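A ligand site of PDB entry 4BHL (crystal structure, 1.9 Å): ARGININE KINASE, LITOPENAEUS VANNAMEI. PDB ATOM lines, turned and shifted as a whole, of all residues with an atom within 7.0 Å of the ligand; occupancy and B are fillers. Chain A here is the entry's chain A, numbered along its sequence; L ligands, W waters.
N of Phe 194 sits at hydrogen-bond distance from OD1 of Asp 192 (3.0 Å).
The side-chain carboxylate (OE2) of Glu 225 lies within hydrogen-bond range of the side-chain amide nitrogen (ND2) of Asn 274, 3.4 Å away.
The side-chain amide oxygen of Asn 274 sits at hydrogen-bond distance from the guanidinium group of Arg 126 (3.1 Å).
The side-chain hydroxyl (OG) of Ser 56 lies within hydrogen-bond range of the backbone carbonyl oxygen (O) of Phe 194, at 2.6 Å.
SG of Cys 271 lies within hydrogen-bond range of OG1 of Thr 273 (3.0 Å).
The side-chain hydroxyl (OG) of Ser 63 lies within hydrogen-bond range of the backbone carbonyl oxygen (O) of Asn 60.
O of Gly 66 is in hydrogen-bond range of N of Gly 57, at 3.0 Å.
Ser 63 touches the ligand (CB to O2, 3.4 Å).
CD1 of Phe 194 touches C1 of the ligand, at 3.8 Å.
Thr 273 touches the ligand (OG1 to C5, 3.7 Å).
ND2 of Asn 274 touches N3 of the ligand (3.9 Å).
Hydrophobic or aromatic side chains within 4 Å of the ligand: Val 65, Tyr 68 and Phe 194.
Ten residues have an atom within 4 Å of the ligand: Ser 63, Gly 64, Val 65, Gly 66, Tyr 68, Phe 194, Glu 225, Cys 271, Thr 273 and Asn 274.
The nearest printed residue that does not touch the ligand is Ser 56 (4.7 Å).
The side-chain sulfur (SG) of Cys 271 sits at hydrogen-bond distance from a nitrogen (N3) of the ligand, at 3.3 Å.
A nitrogen (N3) of the ligand lies within salt-bridge range of the side-chain carboxylate (OE2) of Glu 225, 2.8 Å away.
N of Gly 64 sits at hydrogen-bond distance from O1 of the ligand, at 2.9 Å.
A nitrogen (N1) of the ligand sits at hydrogen-bond distance from the side-chain hydroxyl of Tyr 68, 2.7 Å away.
N of Gly 66 is in hydrogen-bond range of O2 of the ligand, at 2.9 Å.
N of Val 65 lies within hydrogen-bond range of O2 of the ligand, at 2.9 Å.
Water W5 lies within hydrogen-bond range of the side-chain hydroxyl (OG) of Ser 63 (2.7 Å), the side-chain hydroxyl (OG) of Ser 56 (2.8 Å) and a nitrogen (N1) of the ligand (2.9 Å).
Water W3 lies within hydrogen-bond range of the backbone carbonyl oxygen (O) of Ile 67 (2.8 Å), a nitrogen (N1) of the ligand (2.9 Å) and the side-chain sulfur (SG) of Cys 271 (3.3 Å).
Water W4 lies within hydrogen-bond range of OH of Tyr 68, OE1 of Glu 225 and N4 of the ligand.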
ATOM      1  N   SER A  25      33.696 -22.650  -9.332  1.00  0.00           N
ATOM      2  CA  SER A  25      33.426 -23.869  -8.568  1.00  0.00           C
ATOM      3  C   SER A  25      34.688 -24.716  -8.436  1.00  0.00           C
ATOM      4  O   SER A  25      35.566 -24.680  -9.306  1.00  0.00           O
ATOM      5  CB  SER A  25      32.323 -24.704  -9.216  1.00  0.00           C
ATOM      6  OG  SER A  25      32.733 -25.178 -10.490  1.00  0.00           O
ATOM      7  N   SER A  56      25.403 -31.694 -11.234  1.00  0.00           N
ATOM      8  CA  SER A  56      24.901 -30.526 -10.518  1.00  0.00           C
ATOM      9  C   SER A  56      25.777 -29.288 -10.752  1.00  0.00           C
ATOM     10  O   SER A  56      25.254 -28.172 -10.887  1.00  0.00           O
ATOM     11  CB  SER A  56      24.760 -30.808  -9.024  1.00  0.00           C
ATOM     12  OG  SER A  56      24.149 -29.716  -8.366  1.00  0.00           O
ATOM     13  N   GLY A  57      27.091 -29.483 -10.787  1.00  0.00           N
ATOM     14  CA  GLY A  57      28.038 -28.405 -10.995  1.00  0.00           C
ATOM     15  C   GLY A  57      28.074 -27.934 -12.440  1.00  0.00           C
ATOM     16  O   GLY A  57      28.427 -26.776 -12.724  1.00  0.00           O
ATOM     17  N   ASN A  60      24.503 -26.028 -12.609  1.00  0.00           N
ATOM     18  CA  ASN A  60      24.522 -24.834 -11.794  1.00  0.00           C
ATOM     19  C   ASN A  60      25.952 -24.332 -11.733  1.00  0.00           C
ATOM     20  O   ASN A  60      26.717 -24.728 -10.859  1.00  0.00           O
ATOM     21  CB  ASN A  60      24.014 -25.139 -10.392  1.00  0.00           C
ATOM     22  CG  ASN A  60      22.619 -25.734 -10.396  1.00  0.00           C
ATOM     23  OD1 ASN A  60      21.626 -25.022 -10.566  1.00  0.00           O
ATOM     24  ND2 ASN A  60      22.530 -27.041 -10.227  1.00  0.00           N
ATOM     25  N   ASP A  62      27.164 -21.584 -10.874  1.00  0.00           N
ATOM     26  CA  ASP A  62      27.465 -20.810  -9.672  1.00  0.00           C
ATOM     27  C   ASP A  62      27.659 -21.666  -8.426  1.00  0.00           C
ATOM     28  O   ASP A  62      27.736 -21.150  -7.316  1.00  0.00           O
ATOM     29  CB  ASP A  62      26.404 -19.741  -9.413  1.00  0.00           C
ATOM     30  CG  ASP A  62      25.030 -20.325  -9.149  1.00  0.00           C
ATOM     31  OD1 ASP A  62      24.742 -21.425  -9.665  1.00  0.00           O
ATOM     32  OD2 ASP A  62      24.242 -19.682  -8.423  1.00  0.00           O
ATOM     33  N   SER A  63      27.753 -22.986  -8.614  1.00  0.00           N
ATOM     34  CA  SER A  63      28.080 -23.880  -7.510  1.00  0.00           C
ATOM     35  C   SER A  63      29.422 -23.501  -6.868  1.00  0.00           C
ATOM     36  O   SER A  63      30.334 -23.013  -7.539  1.00  0.00           O
ATOM     37  CB  SER A  63      28.131 -25.330  -7.988  1.00  0.00           C
ATOM     38  OG  SER A  63      26.874 -25.756  -8.502  1.00  0.00           O
ATOM     39  N   GLY A  64      29.552 -23.716  -5.561  1.00  0.00           N
ATOM     40  CA  GLY A  64      30.849 -23.492  -4.923  1.00  0.00           C
ATOM     41  C   GLY A  64      31.722 -24.715  -5.117  1.00  0.00           C
ATOM     42  O   GLY A  64      32.939 -24.613  -5.337  1.00  0.00           O
ATOM     43  N   VAL A  65      31.094 -25.879  -5.040  1.00  0.00           N
ATOM     44  CA  VAL A  65      31.798 -27.156  -5.111  1.00  0.00           C
ATOM     45  C   VAL A  65      31.381 -27.857  -6.409  1.00  0.00           C
ATOM     46  O   VAL A  65      32.184 -27.995  -7.313  1.00  0.00           O
ATOM     47  CB  VAL A  65      31.480 -28.015  -3.872  1.00  0.00           C
ATOM     48  CG1 VAL A  65      32.247 -29.336  -3.900  1.00  0.00           C
ATOM     49  CG2 VAL A  65      31.834 -27.229  -2.596  1.00  0.00           C
ATOM     50  N   GLY A  66      30.107 -28.223  -6.514  1.00  0.00           N
ATOM     51  CA  GLY A  66      29.568 -28.685  -7.776  1.00  0.00           C
ATOM     52  C   GLY A  66      29.623 -30.178  -8.044  1.00  0.00           C
ATOM     53  O   GLY A  66      29.332 -30.638  -9.157  1.00  0.00           O
ATOM     54  N   ILE A  67      29.977 -30.966  -7.035  1.00  0.00           N
ATOM     55  CA  ILE A  67      29.901 -32.411  -7.148  1.00  0.00           C
ATOM     56  C   ILE A  67      29.227 -33.040  -5.947  1.00  0.00           C
ATOM     57  O   ILE A  67      29.203 -32.456  -4.860  1.00  0.00           O
ATOM     58  CB  ILE A  67      31.269 -33.058  -7.335  1.00  0.00           C
ATOM     59  CG1 ILE A  67      32.124 -32.916  -6.074  1.00  0.00           C
ATOM     60  CG2 ILE A  67      31.976 -32.492  -8.597  1.00  0.00           C
ATOM     61  CD1 ILE A  67      33.372 -33.792  -6.087  1.00  0.00           C
ATOM     62  N   TYR A  68      28.705 -34.243  -6.154  1.00  0.00           N
ATOM     63  CA  TYR A  68      28.116 -35.048  -5.075  1.00  0.00           C
ATOM     64  C   TYR A  68      28.513 -36.499  -5.304  1.00  0.00           C
ATOM     65  O   TYR A  68      28.827 -36.896  -6.431  1.00  0.00           O
ATOM     66  CB  TYR A  68      26.588 -34.970  -5.138  1.00  0.00           C
ATOM     67  CG  TYR A  68      25.975 -33.619  -4.783  1.00  0.00           C
ATOM     68  CD1 TYR A  68      25.776 -32.642  -5.750  1.00  0.00           C
ATOM     69  CD2 TYR A  68      25.551 -33.346  -3.476  1.00  0.00           C
ATOM     70  CE1 TYR A  68      25.197 -31.423  -5.442  1.00  0.00           C
ATOM     71  CE2 TYR A  68      24.949 -32.105  -3.156  1.00  0.00           C
ATOM     72  CZ  TYR A  68      24.779 -31.156  -4.146  1.00  0.00           C
ATOM     73  OH  TYR A  68      24.202 -29.921  -3.865  1.00  0.00           O
ATOM     74  N   TYR A  89      38.453 -27.762  -0.366  1.00  0.00           N
ATOM     75  CA  TYR A  89      37.309 -27.310   0.439  1.00  0.00           C
ATOM     76  C   TYR A  89      37.617 -27.384   1.937  1.00  0.00           C
ATOM     77  O   TYR A  89      37.428 -26.406   2.663  1.00  0.00           O
ATOM     78  CB  TYR A  89      36.029 -28.117   0.143  1.00  0.00           C
ATOM     79  CG  TYR A  89      34.830 -27.568   0.879  1.00  0.00           C
ATOM     80  CD1 TYR A  89      34.117 -26.490   0.356  1.00  0.00           C
ATOM     81  CD2 TYR A  89      34.443 -28.080   2.116  1.00  0.00           C
ATOM     82  CE1 TYR A  89      33.026 -25.949   1.036  1.00  0.00           C
ATOM     83  CE2 TYR A  89      33.364 -27.546   2.807  1.00  0.00           C
ATOM     84  CZ  TYR A  89      32.654 -26.486   2.260  1.00  0.00           C
ATOM     85  OH  TYR A  89      31.569 -25.951   2.929  1.00  0.00           O
ATOM     86  N   ARG A 126      23.965 -30.143  14.675  1.00  0.00           N
ATOM     87  CA  ARG A 126      23.443 -31.080  13.708  1.00  0.00           C
ATOM     88  C   ARG A 126      24.548 -31.990  13.213  1.00  0.00           C
ATOM     89  O   ARG A 126      25.714 -31.610  13.198  1.00  0.00           O
ATOM     90  CB  ARG A 126      22.803 -30.353  12.529  1.00  0.00           C
ATOM     91  CG  ARG A 126      23.778 -29.945  11.432  1.00  0.00           C
ATOM     92  CD  ARG A 126      23.512 -30.673  10.113  1.00  0.00           C
ATOM     93  NE  ARG A 126      23.986 -29.880   8.979  1.00  0.00           N
ATOM     94  CZ  ARG A 126      24.994 -30.230   8.185  1.00  0.00           C
ATOM     95  NH1 ARG A 126      25.640 -31.374   8.366  1.00  0.00           N
ATOM     96  NH2 ARG A 126      25.347 -29.426   7.189  1.00  0.00           N
ATOM     97  N   ASP A 192      16.361 -27.938  -3.871  1.00  0.00           N
ATOM     98  CA  ASP A 192      16.531 -26.858  -4.832  1.00  0.00           C
ATOM     99  C   ASP A 192      17.259 -27.319  -6.099  1.00  0.00           C
ATOM    100  O   ASP A 192      17.565 -28.502  -6.248  1.00  0.00           O
ATOM    101  CB  ASP A 192      17.260 -25.660  -4.194  1.00  0.00           C
ATOM    102  CG  ASP A 192      18.685 -25.979  -3.758  1.00  0.00           C
ATOM    103  OD1 ASP A 192      19.290 -26.957  -4.244  1.00  0.00           O
ATOM    104  OD2 ASP A 192      19.212 -25.232  -2.920  1.00  0.00           O
ATOM    105  N   PHE A 194      20.279 -27.184  -7.047  1.00  0.00           N
ATOM    106  CA  PHE A 194      21.542 -27.906  -6.864  1.00  0.00           C
ATOM    107  C   PHE A 194      21.263 -29.383  -6.603  1.00  0.00           C
ATOM    108  O   PHE A 194      21.966 -30.255  -7.118  1.00  0.00           O
ATOM    109  CB  PHE A 194      22.359 -27.307  -5.718  1.00  0.00           C
ATOM    110  CG  PHE A 194      22.736 -25.881  -5.932  1.00  0.00           C
ATOM    111  CD1 PHE A 194      23.830 -25.548  -6.702  1.00  0.00           C
ATOM    112  CD2 PHE A 194      21.973 -24.864  -5.382  1.00  0.00           C
ATOM    113  CE1 PHE A 194      24.190 -24.220  -6.912  1.00  0.00           C
ATOM    114  CE2 PHE A 194      22.304 -23.552  -5.579  1.00  0.00           C
ATOM    115  CZ  PHE A 194      23.421 -23.218  -6.356  1.00  0.00           C
ATOM    116  N   LEU A 195      20.237 -29.655  -5.806  1.00  0.00           N
ATOM    117  CA  LEU A 195      19.893 -31.037  -5.492  1.00  0.00           C
ATOM    118  C   LEU A 195      19.154 -31.695  -6.669  1.00  0.00           C
ATOM    119  O   LEU A 195      19.397 -32.859  -6.982  1.00  0.00           O
ATOM    120  CB  LEU A 195      19.072 -31.113  -4.204  1.00  0.00           C
ATOM    121  CG  LEU A 195      19.881 -30.873  -2.927  1.00  0.00           C
ATOM    122  CD1 LEU A 195      18.952 -30.649  -1.743  1.00  0.00           C
ATOM    123  CD2 LEU A 195      20.879 -32.034  -2.657  1.00  0.00           C
ATOM    124  N   GLU A 224      16.240 -35.953   3.070  1.00  0.00           N
ATOM    125  CA  GLU A 224      16.267 -34.613   2.512  1.00  0.00           C
ATOM    126  C   GLU A 224      17.445 -34.433   1.553  1.00  0.00           C
ATOM    127  O   GLU A 224      17.251 -34.265   0.348  1.00  0.00           O
ATOM    128  CB  GLU A 224      16.320 -33.561   3.622  1.00  0.00           C
ATOM    129  CG  GLU A 224      16.301 -32.117   3.113  1.00  0.00           C
ATOM    130  CD  GLU A 224      17.659 -31.428   3.186  1.00  0.00           C
ATOM    131  OE1 GLU A 224      18.554 -31.929   3.911  1.00  0.00           O
ATOM    132  OE2 GLU A 224      17.822 -30.378   2.540  1.00  0.00           O
ATOM    133  N   GLU A 225      18.667 -34.460   2.075  1.00  0.00           N
ATOM    134  CA  GLU A 225      19.869 -34.444   1.237  1.00  0.00           C
ATOM    135  C   GLU A 225      20.691 -35.688   1.581  1.00  0.00           C
ATOM    136  O   GLU A 225      21.142 -36.420   0.711  1.00  0.00           O
ATOM    137  CB  GLU A 225      20.690 -33.173   1.471  1.00  0.00           C
ATOM    138  CG  GLU A 225      22.098 -33.230   0.849  1.00  0.00           C
ATOM    139  CD  GLU A 225      22.856 -31.912   0.958  1.00  0.00           C
ATOM    140  OE1 GLU A 225      22.245 -30.846   0.733  1.00  0.00           O
ATOM    141  OE2 GLU A 225      24.066 -31.932   1.271  1.00  0.00           O
ATOM    142  N   ASP A 226      20.868 -35.923   2.871  1.00  0.00           N
ATOM    143  CA  ASP A 226      21.426 -37.195   3.319  1.00  0.00           C
ATOM    144  C   ASP A 226      20.299 -38.063   3.849  1.00  0.00           C
ATOM    145  O   ASP A 226      19.218 -37.562   4.114  1.00  0.00           O
ATOM    146  CB  ASP A 226      22.474 -36.947   4.410  1.00  0.00           C
ATOM    147  CG  ASP A 226      23.785 -36.447   3.854  1.00  0.00           C
ATOM    148  OD1 ASP A 226      24.389 -37.199   3.069  1.00  0.00           O
ATOM    149  OD2 ASP A 226      24.208 -35.311   4.194  1.00  0.00           O
ATOM    150  N   ARG A 229      19.441 -36.375   8.711  1.00  0.00           N
ATOM    151  CA  ARG A 229      20.012 -35.141   9.215  1.00  0.00           C
ATOM    152  C   ARG A 229      19.478 -35.026  10.632  1.00  0.00           C
ATOM    153  O   ARG A 229      18.273 -34.964  10.841  1.00  0.00           O
ATOM    154  CB  ARG A 229      19.567 -33.932   8.376  1.00  0.00           C
ATOM    155  CG  ARG A 229      20.176 -32.623   8.873  1.00  0.00           C
ATOM    156  CD  ARG A 229      19.630 -31.400   8.134  1.00  0.00           C
ATOM    157  NE  ARG A 229      20.106 -31.324   6.754  1.00  0.00           N
ATOM    158  CZ  ARG A 229      20.355 -30.191   6.112  1.00  0.00           C
ATOM    159  NH1 ARG A 229      20.195 -29.026   6.732  1.00  0.00           N
ATOM    160  NH2 ARG A 229      20.783 -30.214   4.856  1.00  0.00           N
ATOM    161  N   PHE A 270      26.419 -37.262   1.230  1.00  0.00           N
ATOM    162  CA  PHE A 270      26.094 -37.097  -0.187  1.00  0.00           C
ATOM    163  C   PHE A 270      26.950 -35.980  -0.767  1.00  0.00           C
ATOM    164  O   PHE A 270      27.532 -36.138  -1.851  1.00  0.00           O
ATOM    165  CB  PHE A 270      24.600 -36.780  -0.332  1.00  0.00           C
ATOM    166  CG  PHE A 270      24.154 -36.614  -1.759  1.00  0.00           C
ATOM    167  CD1 PHE A 270      24.626 -37.452  -2.745  1.00  0.00           C
ATOM    168  CD2 PHE A 270      23.251 -35.632  -2.098  1.00  0.00           C
ATOM    169  CE1 PHE A 270      24.227 -37.318  -4.046  1.00  0.00           C
ATOM    170  CE2 PHE A 270      22.841 -35.470  -3.404  1.00  0.00           C
ATOM    171  CZ  PHE A 270      23.324 -36.336  -4.385  1.00  0.00           C
ATOM    172  N   CYS A 271      27.033 -34.875  -0.046  1.00  0.00           N
ATOM    173  CA  CYS A 271      27.906 -33.776  -0.460  1.00  0.00           C
ATOM    174  C   CYS A 271      29.237 -33.887   0.280  1.00  0.00           C
ATOM    175  O   CYS A 271      29.255 -34.095   1.496  1.00  0.00           O
ATOM    176  CB  CYS A 271      27.258 -32.424  -0.143  1.00  0.00           C
ATOM    177  SG  CYS A 271      28.302 -31.037  -0.603  1.00  0.00           S
ATOM    178  N   PRO A 272      30.344 -33.744  -0.450  1.00  0.00           N
ATOM    179  CA  PRO A 272      31.623 -33.880   0.233  1.00  0.00           C
ATOM    180  C   PRO A 272      31.883 -32.735   1.225  1.00  0.00           C
ATOM    181  O   PRO A 272      32.792 -32.855   2.045  1.00  0.00           O
ATOM    182  CB  PRO A 272      32.651 -33.886  -0.912  1.00  0.00           C
ATOM    183  CG  PRO A 272      31.919 -33.280  -2.096  1.00  0.00           C
ATOM    184  CD  PRO A 272      30.488 -33.677  -1.912  1.00  0.00           C
ATOM    185  N   THR A 273      31.119 -31.655   1.164  1.00  0.00           N
ATOM    186  CA  THR A 273      31.295 -30.606   2.159  1.00  0.00           C
ATOM    187  C   THR A 273      30.882 -31.077   3.549  1.00  0.00           C
ATOM    188  O   THR A 273      31.236 -30.445   4.537  1.00  0.00           O
ATOM    189  CB  THR A 273      30.492 -29.305   1.863  1.00  0.00           C
ATOM    190  OG1 THR A 273      29.080 -29.578   1.955  1.00  0.00           O
ATOM    191  CG2 THR A 273      30.854 -28.727   0.491  1.00  0.00           C
ATOM    192  N   ASN A 274      30.154 -32.187   3.621  1.00  0.00           N
ATOM    193  CA  ASN A 274      29.605 -32.657   4.892  1.00  0.00           C
ATOM    194  C   ASN A 274      30.325 -33.850   5.524  1.00  0.00           C
ATOM    195  O   ASN A 274      29.811 -34.432   6.482  1.00  0.00           O
ATOM    196  CB  ASN A 274      28.115 -32.963   4.753  1.00  0.00           C
ATOM    197  CG  ASN A 274      27.292 -31.706   4.673  1.00  0.00           C
ATOM    198  OD1 ASN A 274      27.510 -30.754   5.423  1.00  0.00           O
ATOM    199  ND2 ASN A 274      26.324 -31.698   3.752  1.00  0.00           N
HETATM  200  N1  LIG L   1      26.223 -28.250  -4.439  1.00  0.00           N
HETATM  201  C1  LIG L   1      26.120 -26.885  -3.928  1.00  0.00           C
HETATM  202  C2  LIG L   1      27.353 -26.083  -4.299  1.00  0.00           C
HETATM  203  O1  LIG L   1      27.410 -24.876  -4.080  1.00  0.00           O
HETATM  204  C3  LIG L   1      25.945 -26.864  -2.409  1.00  0.00           C
HETATM  205  C4  LIG L   1      26.957 -27.703  -1.672  1.00  0.00           C
HETATM  206  C5  LIG L   1      26.998 -27.375  -0.186  1.00  0.00           C
HETATM  207  N2  LIG L   1      25.650 -27.349   0.386  1.00  0.00           N
HETATM  208  C6  LIG L   1      24.979 -28.432   0.736  1.00  0.00           C
HETATM  209  N3  LIG L   1      25.524 -29.646   0.580  1.00  0.00           N
HETATM  210  N4  LIG L   1      23.756 -28.293   1.253  1.00  0.00           N
HETATM  211  O2  LIG L   1      28.321 -26.651  -4.819  1.00  0.00           O
HETATM  212  O   HOH W   1      24.235 -24.961   0.642  1.00  0.00           O
HETATM  213  O   HOH W   2      25.071 -23.334  -3.253  1.00  0.00           O
HETATM  214  O   HOH W   3      28.471 -29.987  -3.681  1.00  0.00           O
HETATM  215  O   HOH W   4      22.851 -29.432  -1.730  1.00  0.00           O
HETATM  216  O   HOH W   5      26.247 -28.114  -7.305  1.00  0.00           O
